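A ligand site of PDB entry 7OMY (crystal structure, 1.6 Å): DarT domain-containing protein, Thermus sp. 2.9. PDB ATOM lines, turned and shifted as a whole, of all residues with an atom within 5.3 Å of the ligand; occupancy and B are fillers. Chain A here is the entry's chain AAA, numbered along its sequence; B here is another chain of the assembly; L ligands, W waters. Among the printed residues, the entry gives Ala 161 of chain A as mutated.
OG1 of Thr 16 lies within hydrogen-bond range of O6 of the ligand (2.6 Å).
A ring nitrogen (ND1) of His 33 lies within hydrogen-bond range of an oxygen (O2) of the ligand (2.8 Å).
A ring nitrogen (NE2) of His 14 is in hydrogen-bond range of an oxygen (O6) of the ligand (2.8 Å).
A ring nitrogen (NE2) of His 66 sits at hydrogen-bond distance from an oxygen (O11) of the ligand, at 2.8 Å.
N of Ile 15 is in hydrogen-bond range of O13 of the ligand, at 2.9 Å.
O of Ile 15 sits at hydrogen-bond distance from N7 of the ligand (3.1 Å).
The backbone NH (N) of Leu 31 lies within hydrogen-bond range of a nitrogen (N2) of the ligand, at 2.9 Å.
A nitrogen (N3) of the ligand lies within hydrogen-bond range of the backbone carbonyl oxygen (O) of Lys 29 (3.1 Å).
N3 of the ligand lies within hydrogen-bond range of O of Gly 23 (3.3 Å).
The guanidinium group (NE) of Arg 52 lies close to an oxygen (O11) of the ligand, at 3.2 Å.
The backbone NH (N) of Ile 24 lies within hydrogen-bond range of a nitrogen (N4) of the ligand (3.2 Å).
O5 of the ligand sits at hydrogen-bond distance from ND2 of Asn 20 (3.2 Å).
The side-chain hydroxyl of Thr 16 sits at hydrogen-bond distance from the side-chain amide nitrogen of Asn 20 (3.0 Å).
A ring nitrogen (ND1) of His 14 is in hydrogen-bond range of the backbone carbonyl oxygen (O) of Pro 70 (2.7 Å).
N of His 66 is in hydrogen-bond range of O of Arg 52, 3.2 Å away.
The backbone NH of Lys 29 is in hydrogen-bond range of the backbone carbonyl oxygen of Ile 24 (3.1 Å).
O2 of DT 4 of chain B is in hydrogen-bond range of the guanidinium group (NH2) of Arg 52, 2.7 Å away.
N of Gln 40 lies within hydrogen-bond range of OD1 of Asn 20, 2.7 Å away.
O of Tyr 13 lies within hydrogen-bond range of N of Tyr 72 (2.8 Å).
N of Ala 44 sits at hydrogen-bond distance from OG of Ser 42, at 3.4 Å.
O of Tyr 13 touches O13 of the ligand, at 3.8 Å.
Met 27 touches the ligand.
CA of Leu 30 touches N2 of the ligand, at 3.5 Å.
CG of Pro 37 touches O4 of the ligand, at 3.4 Å.
Pro 38 touches the ligand (O to C9, 3.6 Å).
Lys 39 touches the ligand (CA to N5, 3.5 Å).
Ile 43 touches the ligand (CG1 to O8, 3.9 Å).
CB of Ala 44 touches C11 of the ligand, at 3.5 Å.
Pro 70 touches the ligand.
Phe 71 touches the ligand (C to C20, 3.8 Å).
Tyr 72 touches the ligand.
Met 79 touches the ligand (CE to O10, 3.4 Å).
DT 4 of chain B touches the ligand (O4 to C11, 3.6 Å).
Of the 29 residues printed, 24 come within 4 Å of the ligand.
The nearest printed residue that does not touch the ligand is Arg 41 (4.3 Å).
Water W8 lies within hydrogen-bond range of an oxygen (O13) of the ligand (2.5 Å), the backbone carbonyl oxygen of Tyr 13 (2.6 Å) and the backbone NH of Ile 15 (3.4 Å).
Water W5 lies within hydrogen-bond range of an oxygen (O8) of the ligand and the backbone NH of Ile 43.
Water W6 lies within hydrogen-bond range of an oxygen (O11) of the ligand (2.6 Å) and a ring nitrogen (NE2) of His 66 (3.4 Å).
Water W4 lies within hydrogen-bond range of OG of Ser 42, O1 of the ligand and NZ of Lys 39.
Water W10 lies within hydrogen-bond range of O5 of the ligand (2.7 Å) and O of Ile 15 (2.7 Å).
Water W1 lies within hydrogen-bond range of N of His 17, ND2 of Asn 20, O5 of the ligand, O of Arg 41 and OG1 of Thr 16.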
ATOM      1  N   TYR A  13      11.700 -31.892  -0.282  1.00  0.00           N
ATOM      2  CA  TYR A  13      12.062 -32.882  -1.302  1.00  0.00           C
ATOM      3  C   TYR A  13      12.056 -32.221  -2.671  1.00  0.00           C
ATOM      4  O   TYR A  13      11.019 -31.697  -3.087  1.00  0.00           O
ATOM      5  CB  TYR A  13      11.089 -34.062  -1.350  1.00  0.00           C
ATOM      6  CG  TYR A  13      10.876 -34.750  -0.039  1.00  0.00           C
ATOM      7  CD1 TYR A  13       9.979 -34.253   0.877  1.00  0.00           C
ATOM      8  CD2 TYR A  13      11.569 -35.914   0.275  1.00  0.00           C
ATOM      9  CE1 TYR A  13       9.804 -34.864   2.107  1.00  0.00           C
ATOM     10  CE2 TYR A  13      11.352 -36.564   1.477  1.00  0.00           C
ATOM     11  CZ  TYR A  13      10.491 -36.011   2.398  1.00  0.00           C
ATOM     12  OH  TYR A  13      10.260 -36.650   3.585  1.00  0.00           O
ATOM     13  N   HIS A  14      13.166 -32.322  -3.395  1.00  0.00           N
ATOM     14  CA  HIS A  14      13.280 -31.880  -4.823  1.00  0.00           C
ATOM     15  C   HIS A  14      13.610 -33.123  -5.649  1.00  0.00           C
ATOM     16  O   HIS A  14      14.674 -33.708  -5.424  1.00  0.00           O
ATOM     17  CB  HIS A  14      14.344 -30.804  -4.954  1.00  0.00           C
ATOM     18  CG  HIS A  14      14.577 -30.341  -6.356  1.00  0.00           C
ATOM     19  ND1 HIS A  14      13.878 -29.283  -6.905  1.00  0.00           N
ATOM     20  CD2 HIS A  14      15.394 -30.834  -7.332  1.00  0.00           C
ATOM     21  CE1 HIS A  14      14.314 -29.130  -8.180  1.00  0.00           C
ATOM     22  NE2 HIS A  14      15.224 -30.077  -8.442  1.00  0.00           N
ATOM     23  N   ILE A  15      12.777 -33.459  -6.629  1.00  0.00           N
ATOM     24  CA  ILE A  15      13.097 -34.568  -7.568  1.00  0.00           C
ATOM     25  C   ILE A  15      13.811 -34.012  -8.787  1.00  0.00           C
ATOM     26  O   ILE A  15      13.496 -32.943  -9.281  1.00  0.00           O
ATOM     27  CB  ILE A  15      11.890 -35.405  -7.947  1.00  0.00           C
ATOM     28  CG1 ILE A  15      10.702 -34.586  -8.459  1.00  0.00           C
ATOM     29  CG2 ILE A  15      11.464 -36.246  -6.731  1.00  0.00           C
ATOM     30  CD1 ILE A  15       9.645 -35.460  -9.077  1.00  0.00           C
ATOM     31  N   THR A  16      14.821 -34.736  -9.168  1.00  0.00           N
ATOM     32  CA  THR A  16      15.563 -34.426 -10.425  1.00  0.00           C
ATOM     33  C   THR A  16      16.069 -35.722 -11.039  1.00  0.00           C
ATOM     34  O   THR A  16      16.243 -36.722 -10.336  1.00  0.00           O
ATOM     35  CB  THR A  16      16.641 -33.370 -10.175  1.00  0.00           C
ATOM     36  OG1 THR A  16      16.962 -32.786 -11.470  1.00  0.00           O
ATOM     37  CG2 THR A  16      17.856 -33.917  -9.465  1.00  0.00           C
ATOM     38  N   HIS A  17      16.352 -35.666 -12.334  1.00  0.00           N
ATOM     39  CA  HIS A  17      16.941 -36.801 -13.081  1.00  0.00           C
ATOM     40  C   HIS A  17      18.401 -36.881 -12.701  1.00  0.00           C
ATOM     41  O   HIS A  17      19.051 -35.847 -12.598  1.00  0.00           O
ATOM     42  CB  HIS A  17      16.743 -36.599 -14.576  1.00  0.00           C
ATOM     43  CG  HIS A  17      16.966 -37.837 -15.392  1.00  0.00           C
ATOM     44  ND1 HIS A  17      18.234 -38.321 -15.668  1.00  0.00           N
ATOM     45  CD2 HIS A  17      16.099 -38.711 -15.963  1.00  0.00           C
ATOM     46  CE1 HIS A  17      18.127 -39.377 -16.432  1.00  0.00           C
ATOM     47  NE2 HIS A  17      16.806 -39.645 -16.638  1.00  0.00           N
ATOM     48  N   ASN A  20      21.141 -34.750 -14.236  1.00  0.00           N
ATOM     49  CA  ASN A  20      21.288 -33.338 -13.804  1.00  0.00           C
ATOM     50  C   ASN A  20      22.250 -33.206 -12.624  1.00  0.00           C
ATOM     51  O   ASN A  20      22.599 -32.044 -12.310  1.00  0.00           O
ATOM     52  CB  ASN A  20      19.936 -32.749 -13.475  1.00  0.00           C
ATOM     53  CG  ASN A  20      19.009 -32.705 -14.673  1.00  0.00           C
ATOM     54  OD1 ASN A  20      19.459 -32.642 -15.824  1.00  0.00           O
ATOM     55  ND2 ASN A  20      17.694 -32.656 -14.415  1.00  0.00           N
ATOM     56  N   GLY A  23      25.639 -31.239 -13.065  1.00  0.00           N
ATOM     57  CA  GLY A  23      25.438 -29.793 -13.185  1.00  0.00           C
ATOM     58  C   GLY A  23      25.202 -29.172 -11.824  1.00  0.00           C
ATOM     59  O   GLY A  23      25.650 -28.010 -11.593  1.00  0.00           O
ATOM     60  N   ILE A  24      24.386 -29.841 -11.011  1.00  0.00           N
ATOM     61  CA  ILE A  24      24.118 -29.311  -9.663  1.00  0.00           C
ATOM     62  C   ILE A  24      25.432 -29.275  -8.877  1.00  0.00           C
ATOM     63  O   ILE A  24      25.723 -28.289  -8.198  1.00  0.00           O
ATOM     64  CB  ILE A  24      23.043 -30.184  -8.984  1.00  0.00           C
ATOM     65  CG1 ILE A  24      21.727 -30.059  -9.756  1.00  0.00           C
ATOM     66  CG2 ILE A  24      22.894 -29.783  -7.537  1.00  0.00           C
ATOM     67  CD1 ILE A  24      20.694 -31.152  -9.349  1.00  0.00           C
ATOM     68  N   MET A  27      27.836 -26.505 -10.338  1.00  0.00           N
ATOM     69  CA  MET A  27      27.417 -25.118  -9.969  1.00  0.00           C
ATOM     70  C   MET A  27      27.504 -24.953  -8.453  1.00  0.00           C
ATOM     71  O   MET A  27      27.499 -23.814  -7.985  1.00  0.00           O
ATOM     72  CB  MET A  27      25.995 -24.775 -10.451  1.00  0.00           C
ATOM     73  CG  MET A  27      25.755 -24.700 -12.031  1.00  0.00           C
ATOM     74  SD  MET A  27      26.848 -23.477 -12.861  1.00  0.00           S
ATOM     75  CE  MET A  27      28.207 -24.494 -13.444  1.00  0.00           C
ATOM     76  N   LYS A  29      24.994 -25.772  -6.567  1.00  0.00           N
ATOM     77  CA  LYS A  29      23.647 -25.331  -6.189  1.00  0.00           C
ATOM     78  C   LYS A  29      22.620 -25.785  -7.186  1.00  0.00           C
ATOM     79  O   LYS A  29      22.962 -25.979  -8.327  1.00  0.00           O
ATOM     80  CB  LYS A  29      23.601 -23.817  -6.093  1.00  0.00           C
ATOM     81  CG  LYS A  29      23.999 -23.048  -7.328  1.00  0.00           C
ATOM     82  CD  LYS A  29      24.208 -21.570  -7.006  1.00  0.00           C
ATOM     83  CE  LYS A  29      25.584 -21.184  -6.599  1.00  0.00           C
ATOM     84  NZ  LYS A  29      25.755 -19.703  -6.527  1.00  0.00           N
ATOM     85  N   LEU A  30      21.389 -25.909  -6.734  1.00  0.00           N
ATOM     86  CA  LEU A  30      20.218 -25.946  -7.610  1.00  0.00           C
ATOM     87  C   LEU A  30      19.924 -24.516  -8.024  1.00  0.00           C
ATOM     88  O   LEU A  30      19.964 -23.600  -7.163  1.00  0.00           O
ATOM     89  CB  LEU A  30      19.011 -26.548  -6.887  1.00  0.00           C
ATOM     90  CG  LEU A  30      19.009 -28.050  -6.568  1.00  0.00           C
ATOM     91  CD1 LEU A  30      17.972 -28.372  -5.469  1.00  0.00           C
ATOM     92  CD2 LEU A  30      18.616 -28.829  -7.766  1.00  0.00           C
ATOM     93  N   LEU A  31      19.613 -24.329  -9.284  1.00  0.00           N
ATOM     94  CA  LEU A  31      19.216 -22.995  -9.801  1.00  0.00           C
ATOM     95  C   LEU A  31      17.718 -23.015 -10.155  1.00  0.00           C
ATOM     96  O   LEU A  31      17.207 -24.006 -10.707  1.00  0.00           O
ATOM     97  CB  LEU A  31      20.069 -22.663 -11.038  1.00  0.00           C
ATOM     98  CG  LEU A  31      21.526 -22.350 -10.777  1.00  0.00           C
ATOM     99  CD1 LEU A  31      22.312 -22.281 -12.075  1.00  0.00           C
ATOM    100  CD2 LEU A  31      21.726 -21.070  -9.955  1.00  0.00           C
ATOM    101  N   HIS A  33      14.368 -22.127 -12.267  1.00  0.00           N
ATOM    102  CA  HIS A  33      14.081 -22.212 -13.727  1.00  0.00           C
ATOM    103  C   HIS A  33      14.545 -20.924 -14.430  1.00  0.00           C
ATOM    104  O   HIS A  33      15.169 -20.991 -15.520  1.00  0.00           O
ATOM    105  CB  HIS A  33      12.601 -22.393 -13.849  1.00  0.00           C
ATOM    106  CG  HIS A  33      12.102 -22.448 -15.241  1.00  0.00           C
ATOM    107  ND1 HIS A  33      11.627 -23.605 -15.753  1.00  0.00           N
ATOM    108  CD2 HIS A  33      11.927 -21.488 -16.163  1.00  0.00           C
ATOM    109  CE1 HIS A  33      11.219 -23.373 -16.998  1.00  0.00           C
ATOM    110  NE2 HIS A  33      11.417 -22.073 -17.276  1.00  0.00           N
ATOM    111  N   PRO A  37      19.120 -23.280 -15.378  1.00  0.00           N
ATOM    112  CA  PRO A  37      19.997 -24.353 -14.901  1.00  0.00           C
ATOM    113  C   PRO A  37      20.556 -25.128 -16.070  1.00  0.00           C
ATOM    114  O   PRO A  37      19.785 -25.390 -16.995  1.00  0.00           O
ATOM    115  CB  PRO A  37      19.041 -25.271 -14.118  1.00  0.00           C
ATOM    116  CG  PRO A  37      17.666 -24.809 -14.404  1.00  0.00           C
ATOM    117  CD  PRO A  37      17.760 -23.361 -14.816  1.00  0.00           C
ATOM    118  N   PRO A  38      21.808 -25.605 -15.971  1.00  0.00           N
ATOM    119  CA  PRO A  38      22.442 -26.387 -17.057  1.00  0.00           C
ATOM    120  C   PRO A  38      21.978 -27.853 -16.985  1.00  0.00           C
ATOM    121  O   PRO A  38      22.792 -28.810 -16.885  1.00  0.00           O
ATOM    122  CB  PRO A  38      23.932 -26.176 -16.797  1.00  0.00           C
ATOM    123  CG  PRO A  38      24.020 -26.020 -15.315  1.00  0.00           C
ATOM    124  CD  PRO A  38      22.772 -25.214 -14.945  1.00  0.00           C
ATOM    125  N   LYS A  39      20.661 -28.027 -17.056  1.00  0.00           N
ATOM    126  CA  LYS A  39      20.078 -29.397 -16.953  1.00  0.00           C
ATOM    127  C   LYS A  39      20.375 -30.199 -18.224  1.00  0.00           C
ATOM    128  O   LYS A  39      20.497 -29.583 -19.300  1.00  0.00           O
ATOM    129  CB  LYS A  39      18.581 -29.334 -16.768  1.00  0.00           C
ATOM    130  CG  LYS A  39      17.773 -28.735 -17.904  1.00  0.00           C
ATOM    131  CD  LYS A  39      16.322 -28.427 -17.613  1.00  0.00           C
ATOM    132  CE  LYS A  39      15.670 -27.784 -18.821  1.00  0.00           C
ATOM    133  NZ  LYS A  39      14.257 -27.482 -18.514  1.00  0.00           N
ATOM    134  N   GLN A  40      20.479 -31.514 -18.084  1.00  0.00           N
ATOM    135  CA  GLN A  40      20.616 -32.438 -19.216  1.00  0.00           C
ATOM    136  C   GLN A  40      19.264 -33.048 -19.570  1.00  0.00           C
ATOM    137  O   GLN A  40      19.100 -33.557 -20.656  1.00  0.00           O
ATOM    138  CB  GLN A  40      21.601 -33.543 -18.869  1.00  0.00           C
ATOM    139  CG  GLN A  40      23.028 -33.063 -18.774  1.00  0.00           C
ATOM    140  CD  GLN A  40      23.549 -32.543 -20.105  1.00  0.00           C
ATOM    141  OE1 GLN A  40      23.236 -33.068 -21.177  1.00  0.00           O
ATOM    142  NE2 GLN A  40      24.295 -31.462 -20.028  1.00  0.00           N
ATOM    143  N   ARG A  41      18.312 -33.069 -18.631  1.00  0.00           N
ATOM    144  CA  ARG A  41      17.065 -33.857 -18.837  1.00  0.00           C
ATOM    145  C   ARG A  41      15.915 -33.064 -18.247  1.00  0.00           C
ATOM    146  O   ARG A  41      16.013 -32.684 -17.015  1.00  0.00           O
ATOM    147  CB  ARG A  41      17.197 -35.213 -18.168  1.00  0.00           C
ATOM    148  CG  ARG A  41      16.179 -36.211 -18.695  1.00  0.00           C
ATOM    149  CD  ARG A  41      16.669 -36.828 -19.978  1.00  0.00           C
ATOM    150  NE  ARG A  41      18.023 -37.330 -19.885  1.00  0.00           N
ATOM    151  CZ  ARG A  41      18.719 -37.717 -20.926  1.00  0.00           C
ATOM    152  NH1 ARG A  41      19.957 -38.144 -20.806  1.00  0.00           N
ATOM    153  NH2 ARG A  41      18.152 -37.685 -22.104  1.00  0.00           N
ATOM    154  N   SER A  42      14.871 -32.830 -19.059  1.00  0.00           N
ATOM    155  CA  SER A  42      13.620 -32.215 -18.564  1.00  0.00           C
ATOM    156  C   SER A  42      12.658 -33.331 -18.187  1.00  0.00           C
ATOM    157  O   SER A  42      12.337 -34.189 -19.068  1.00  0.00           O
ATOM    158  CB  SER A  42      13.003 -31.253 -19.496  1.00  0.00           C
ATOM    159  OG  SER A  42      11.709 -30.862 -19.008  1.00  0.00           O
ATOM    160  N   ILE A  43      12.164 -33.345 -16.957  1.00  0.00           N
ATOM    161  CA  ILE A  43      11.071 -34.291 -16.561  1.00  0.00           C
ATOM    162  C   ILE A  43       9.735 -33.560 -16.328  1.00  0.00           C
ATOM    163  O   ILE A  43       8.827 -34.172 -15.722  1.00  0.00           O
ATOM    164  CB  ILE A  43      11.559 -35.094 -15.344  1.00  0.00           C
ATOM    165  CG1 ILE A  43      11.745 -34.226 -14.097  1.00  0.00           C
ATOM    166  CG2 ILE A  43      12.833 -35.878 -15.731  1.00  0.00           C
ATOM    167  CD1 ILE A  43      12.169 -34.954 -12.840  1.00  0.00           C
ATOM    168  N   ALA A  44       9.575 -32.346 -16.820  1.00  0.00           N
ATOM    169  CA  ALA A  44       8.368 -31.525 -16.620  1.00  0.00           C
ATOM    170  C   ALA A  44       7.376 -31.737 -17.764  1.00  0.00           C
ATOM    171  O   ALA A  44       7.765 -32.098 -18.895  1.00  0.00           O
ATOM    172  CB  ALA A  44       8.728 -30.077 -16.553  1.00  0.00           C
ATOM    173  N   ARG A  52       3.806 -20.921 -14.568  1.00  0.00           N
ATOM    174  CA  ARG A  52       4.809 -20.695 -13.487  1.00  0.00           C
ATOM    175  C   ARG A  52       5.682 -19.493 -13.807  1.00  0.00           C
ATOM    176  O   ARG A  52       6.295 -18.894 -12.897  1.00  0.00           O
ATOM    177  CB  ARG A  52       5.685 -21.933 -13.271  1.00  0.00           C
ATOM    178  CG  ARG A  52       5.107 -22.940 -12.281  1.00  0.00           C
ATOM    179  CD  ARG A  52       4.594 -24.198 -12.898  1.00  0.00           C
ATOM    180  NE  ARG A  52       4.159 -25.170 -11.896  1.00  0.00           N
ATOM    181  CZ  ARG A  52       4.005 -26.464 -12.094  1.00  0.00           C
ATOM    182  NH1 ARG A  52       4.150 -26.974 -13.293  1.00  0.00           N
ATOM    183  NH2 ARG A  52       3.666 -27.259 -11.092  1.00  0.00           N
ATOM    184  N   HIS A  66       8.824 -19.415 -11.034  1.00  0.00           N
ATOM    185  CA  HIS A  66      10.045 -19.908 -11.665  1.00  0.00           C
ATOM    186  C   HIS A  66      11.259 -19.080 -11.278  1.00  0.00           C
ATOM    187  O   HIS A  66      12.312 -19.423 -11.740  1.00  0.00           O
ATOM    188  CB  HIS A  66       9.796 -20.053 -13.164  1.00  0.00           C
ATOM    189  CG  HIS A  66       9.308 -21.423 -13.472  1.00  0.00           C
ATOM    190  ND1 HIS A  66       8.771 -21.713 -14.696  1.00  0.00           N
ATOM    191  CD2 HIS A  66       9.118 -22.519 -12.672  1.00  0.00           C
ATOM    192  CE1 HIS A  66       8.362 -22.985 -14.685  1.00  0.00           C
ATOM    193  NE2 HIS A  66       8.566 -23.523 -13.455  1.00  0.00           N
ATOM    194  N   PRO A  70      12.098 -25.199  -6.372  1.00  0.00           N
ATOM    195  CA  PRO A  70      10.913 -25.795  -5.778  1.00  0.00           C
ATOM    196  C   PRO A  70      11.189 -27.114  -5.083  1.00  0.00           C
ATOM    197  O   PRO A  70      12.045 -27.883  -5.494  1.00  0.00           O
ATOM    198  CB  PRO A  70      10.033 -26.042  -7.008  1.00  0.00           C
ATOM    199  CG  PRO A  70      11.019 -26.449  -8.038  1.00  0.00           C
ATOM    200  CD  PRO A  70      12.211 -25.546  -7.801  1.00  0.00           C
ATOM    201  N   PHE A  71      10.437 -27.315  -4.005  1.00  0.00           N
ATOM    202  CA  PHE A  71      10.420 -28.567  -3.213  1.00  0.00           C
ATOM    203  C   PHE A  71       8.985 -28.898  -2.853  1.00  0.00           C
ATOM    204  O   PHE A  71       8.193 -27.975  -2.717  1.00  0.00           O
ATOM    205  CB  PHE A  71      11.184 -28.412  -1.901  1.00  0.00           C
ATOM    206  CG  PHE A  71      12.644 -28.134  -2.014  1.00  0.00           C
ATOM    207  CD1 PHE A  71      13.085 -26.876  -2.370  1.00  0.00           C
ATOM    208  CD2 PHE A  71      13.586 -29.150  -1.771  1.00  0.00           C
ATOM    209  CE1 PHE A  71      14.462 -26.640  -2.475  1.00  0.00           C
ATOM    210  CE2 PHE A  71      14.932 -28.895  -1.867  1.00  0.00           C
ATOM    211  CZ  PHE A  71      15.381 -27.637  -2.218  1.00  0.00           C
ATOM    212  N   TYR A  72       8.675 -30.173  -2.758  1.00  0.00           N
ATOM    213  CA  TYR A  72       7.472 -30.650  -2.081  1.00  0.00           C
ATOM    214  C   TYR A  72       7.787 -30.973  -0.635  1.00  0.00           C
ATOM    215  O   TYR A  72       8.965 -31.026  -0.225  1.00  0.00           O
ATOM    216  CB  TYR A  72       6.845 -31.835  -2.810  1.00  0.00           C
ATOM    217  CG  TYR A  72       6.347 -31.510  -4.195  1.00  0.00           C
ATOM    218  CD1 TYR A  72       5.345 -30.569  -4.413  1.00  0.00           C
ATOM    219  CD2 TYR A  72       6.828 -32.221  -5.304  1.00  0.00           C
ATOM    220  CE1 TYR A  72       4.861 -30.305  -5.687  1.00  0.00           C
ATOM    221  CE2 TYR A  72       6.403 -31.920  -6.589  1.00  0.00           C
ATOM    222  CZ  TYR A  72       5.406 -30.981  -6.763  1.00  0.00           C
ATOM    223  OH  TYR A  72       4.909 -30.743  -8.022  1.00  0.00           O
ATOM    224  N   MET A  79       3.624 -35.388  -9.356  1.00  0.00           N
ATOM    225  CA  MET A  79       4.565 -35.113 -10.480  1.00  0.00           C
ATOM    226  C   MET A  79       5.344 -36.403 -10.807  1.00  0.00           C
ATOM    227  O   MET A  79       5.401 -36.829 -11.999  1.00  0.00           O
ATOM    228  CB  MET A  79       5.525 -33.973 -10.167  1.00  0.00           C
ATOM    229  CG  MET A  79       6.633 -33.857 -11.225  1.00  0.00           C
ATOM    230  SD  MET A  79       7.698 -32.479 -10.735  1.00  0.00           S
ATOM    231  CE  MET A  79       9.042 -32.773 -11.886  1.00  0.00           C
ATOM    232  N   ALA A 161       4.145 -26.522  -1.665  1.00  0.00           N
ATOM    233  CA  ALA A 161       5.554 -26.391  -2.055  1.00  0.00           C
ATOM    234  C   ALA A 161       6.332 -25.467  -1.127  1.00  0.00           C
ATOM    235  O   ALA A 161       5.750 -24.451  -0.614  1.00  0.00           O
ATOM    236  CB  ALA A 161       5.622 -25.937  -3.470  1.00  0.00           C
ATOM    237  P    DT B   4      -1.314 -35.712 -13.921  1.00  0.00           P
ATOM    238  OP1  DT B   4      -2.663 -35.378 -13.464  1.00  0.00           O
ATOM    239  OP2  DT B   4      -0.951 -35.358 -15.303  1.00  0.00           O
ATOM    240  O5'  DT B   4      -0.188 -35.059 -13.010  1.00  0.00           O
ATOM    241  C5'  DT B   4      -0.320 -35.107 -11.582  1.00  0.00           C
ATOM    242  C4'  DT B   4      -0.008 -33.745 -11.023  1.00  0.00           C
ATOM    243  O4'  DT B   4       1.371 -33.383 -11.305  1.00  0.00           O
ATOM    244  C3'  DT B   4      -0.891 -32.629 -11.638  1.00  0.00           C
ATOM    245  O3'  DT B   4      -1.447 -31.809 -10.588  1.00  0.00           O
ATOM    246  C2'  DT B   4       0.120 -31.746 -12.381  1.00  0.00           C
ATOM    247  C1'  DT B   4       1.380 -32.012 -11.593  1.00  0.00           C
ATOM    248  N1   DT B   4       2.564 -31.695 -12.389  1.00  0.00           N
ATOM    249  C2   DT B   4       2.932 -30.367 -12.425  1.00  0.00           C
ATOM    250  O2   DT B   4       2.414 -29.511 -11.724  1.00  0.00           O
ATOM    251  N3   DT B   4       4.015 -30.094 -13.237  1.00  0.00           N
ATOM    252  C4   DT B   4       4.718 -30.989 -14.021  1.00  0.00           C
ATOM    253  O4   DT B   4       5.631 -30.578 -14.765  1.00  0.00           O
ATOM    254  C5   DT B   4       4.280 -32.362 -13.928  1.00  0.00           C
ATOM    255  C7   DT B   4       4.997 -33.400 -14.723  1.00  0.00           C
ATOM    256  C6   DT B   4       3.221 -32.638 -13.148  1.00  0.00           C
HETATM  257  P1  LIG L   1      11.880 -27.128 -14.438  1.00  0.00           P
HETATM  258  O1  LIG L   1      11.044 -27.574 -15.623  1.00  0.00           O
HETATM  259  O2  LIG L   1      11.954 -25.710 -13.958  1.00  0.00           O
HETATM  260  O3  LIG L   1      13.315 -27.783 -14.564  1.00  0.00           O
HETATM  261  C1  LIG L   1      14.498 -27.288 -13.873  1.00  0.00           C
HETATM  262  C2  LIG L   1      15.418 -28.479 -13.864  1.00  0.00           C
HETATM  263  O4  LIG L   1      16.784 -28.031 -13.605  1.00  0.00           O
HETATM  264  C3  LIG L   1      15.121 -29.488 -12.747  1.00  0.00           C
HETATM  265  O5  LIG L   1      15.298 -30.801 -13.256  1.00  0.00           O
HETATM  266  C4  LIG L   1      16.206 -29.144 -11.718  1.00  0.00           C
HETATM  267  O6  LIG L   1      16.561 -30.241 -10.896  1.00  0.00           O
HETATM  268  C5  LIG L   1      17.362 -28.865 -12.662  1.00  0.00           C
HETATM  269  N1  LIG L   1      18.492 -28.190 -12.106  1.00  0.00           N
HETATM  270  C6  LIG L   1      18.508 -27.155 -11.205  1.00  0.00           C
HETATM  271  N2  LIG L   1      19.703 -26.718 -10.937  1.00  0.00           N
HETATM  272  C7  LIG L   1      20.535 -27.441 -11.798  1.00  0.00           C
HETATM  273  C8  LIG L   1      21.926 -27.389 -12.002  1.00  0.00           C
HETATM  274  N3  LIG L   1      22.736 -26.555 -11.340  1.00  0.00           N
HETATM  275  N4  LIG L   1      22.450 -28.225 -12.926  1.00  0.00           N
HETATM  276  C9  LIG L   1      21.610 -29.085 -13.548  1.00  0.00           C
HETATM  277  N5  LIG L   1      20.279 -29.233 -13.432  1.00  0.00           N
HETATM  278  C10 LIG L   1      19.805 -28.377 -12.505  1.00  0.00           C
HETATM  279  O7  LIG L   1      11.307 -27.928 -13.138  1.00  0.00           O
HETATM  280  P2  LIG L   1      11.098 -29.395 -12.555  1.00  0.00           P
HETATM  281  O8  LIG L   1      11.372 -30.322 -13.704  1.00  0.00           O
HETATM  282  O9  LIG L   1      11.847 -29.524 -11.259  1.00  0.00           O
HETATM  283  O10 LIG L   1       9.555 -29.431 -12.248  1.00  0.00           O
HETATM  284  C11 LIG L   1       8.531 -29.231 -13.188  1.00  0.00           C
HETATM  285  C12 LIG L   1       7.584 -28.219 -12.589  1.00  0.00           C
HETATM  286  C13 LIG L   1       6.981 -28.665 -11.242  1.00  0.00           C
HETATM  287  C14 LIG L   1       8.215 -26.849 -12.372  1.00  0.00           C
HETATM  288  O11 LIG L   1       7.215 -25.854 -12.622  1.00  0.00           O
HETATM  289  C15 LIG L   1       8.673 -26.961 -10.918  1.00  0.00           C
HETATM  290  O12 LIG L   1       8.844 -25.642 -10.457  1.00  0.00           O
HETATM  291  C16 LIG L   1       7.511 -27.654 -10.179  1.00  0.00           C
HETATM  292  N6  LIG L   1       7.900 -28.334  -8.888  1.00  0.00           N
HETATM  293  C17 LIG L   1       8.927 -29.247  -8.936  1.00  0.00           C
HETATM  294  C18 LIG L   1       9.371 -29.851  -7.765  1.00  0.00           C
HETATM  295  C19 LIG L   1      10.532 -30.808  -7.828  1.00  0.00           C
HETATM  296  O13 LIG L   1      10.652 -31.569  -6.869  1.00  0.00           O
HETATM  297  N7  LIG L   1      11.379 -30.775  -8.860  1.00  0.00           N
HETATM  298  C20 LIG L   1       8.777 -29.552  -6.549  1.00  0.00           C
HETATM  299  C21 LIG L   1       7.740 -28.648  -6.505  1.00  0.00           C
HETATM  300  C22 LIG L   1       7.299 -28.095  -7.667  1.00  0.00           C
HETATM  301  O   HOH W   1      14.906 -33.757 -14.100  1.00  0.00           O
HETATM  302  O   HOH W   2      15.634 -26.063  -9.676  1.00  0.00           O
HETATM  303  O   HOH W   3       7.250 -23.804  -9.370  1.00  0.00           O
HETATM  304  O   HOH W   4      12.426 -29.245 -17.100  1.00  0.00           O
HETATM  305  O   HOH W   5      13.145 -31.127 -15.329  1.00  0.00           O
HETATM  306  O   HOH W   6       6.954 -25.958 -15.224  1.00  0.00           O
HETATM  307  O   HOH W   7      13.209 -27.098 -10.629  1.00  0.00           O
HETATM  308  O   HOH W   8       9.803 -33.039  -5.012  1.00  0.00           O
HETATM  309  O   HOH W   9       9.280 -26.131 -16.761  1.00  0.00           O
HETATM  310  O   HOH W  10      13.422 -32.055 -11.866  1.00  0.00           O
HETATM  311  O   HOH W  11      11.527 -25.151 -11.374  1.00  0.00           O
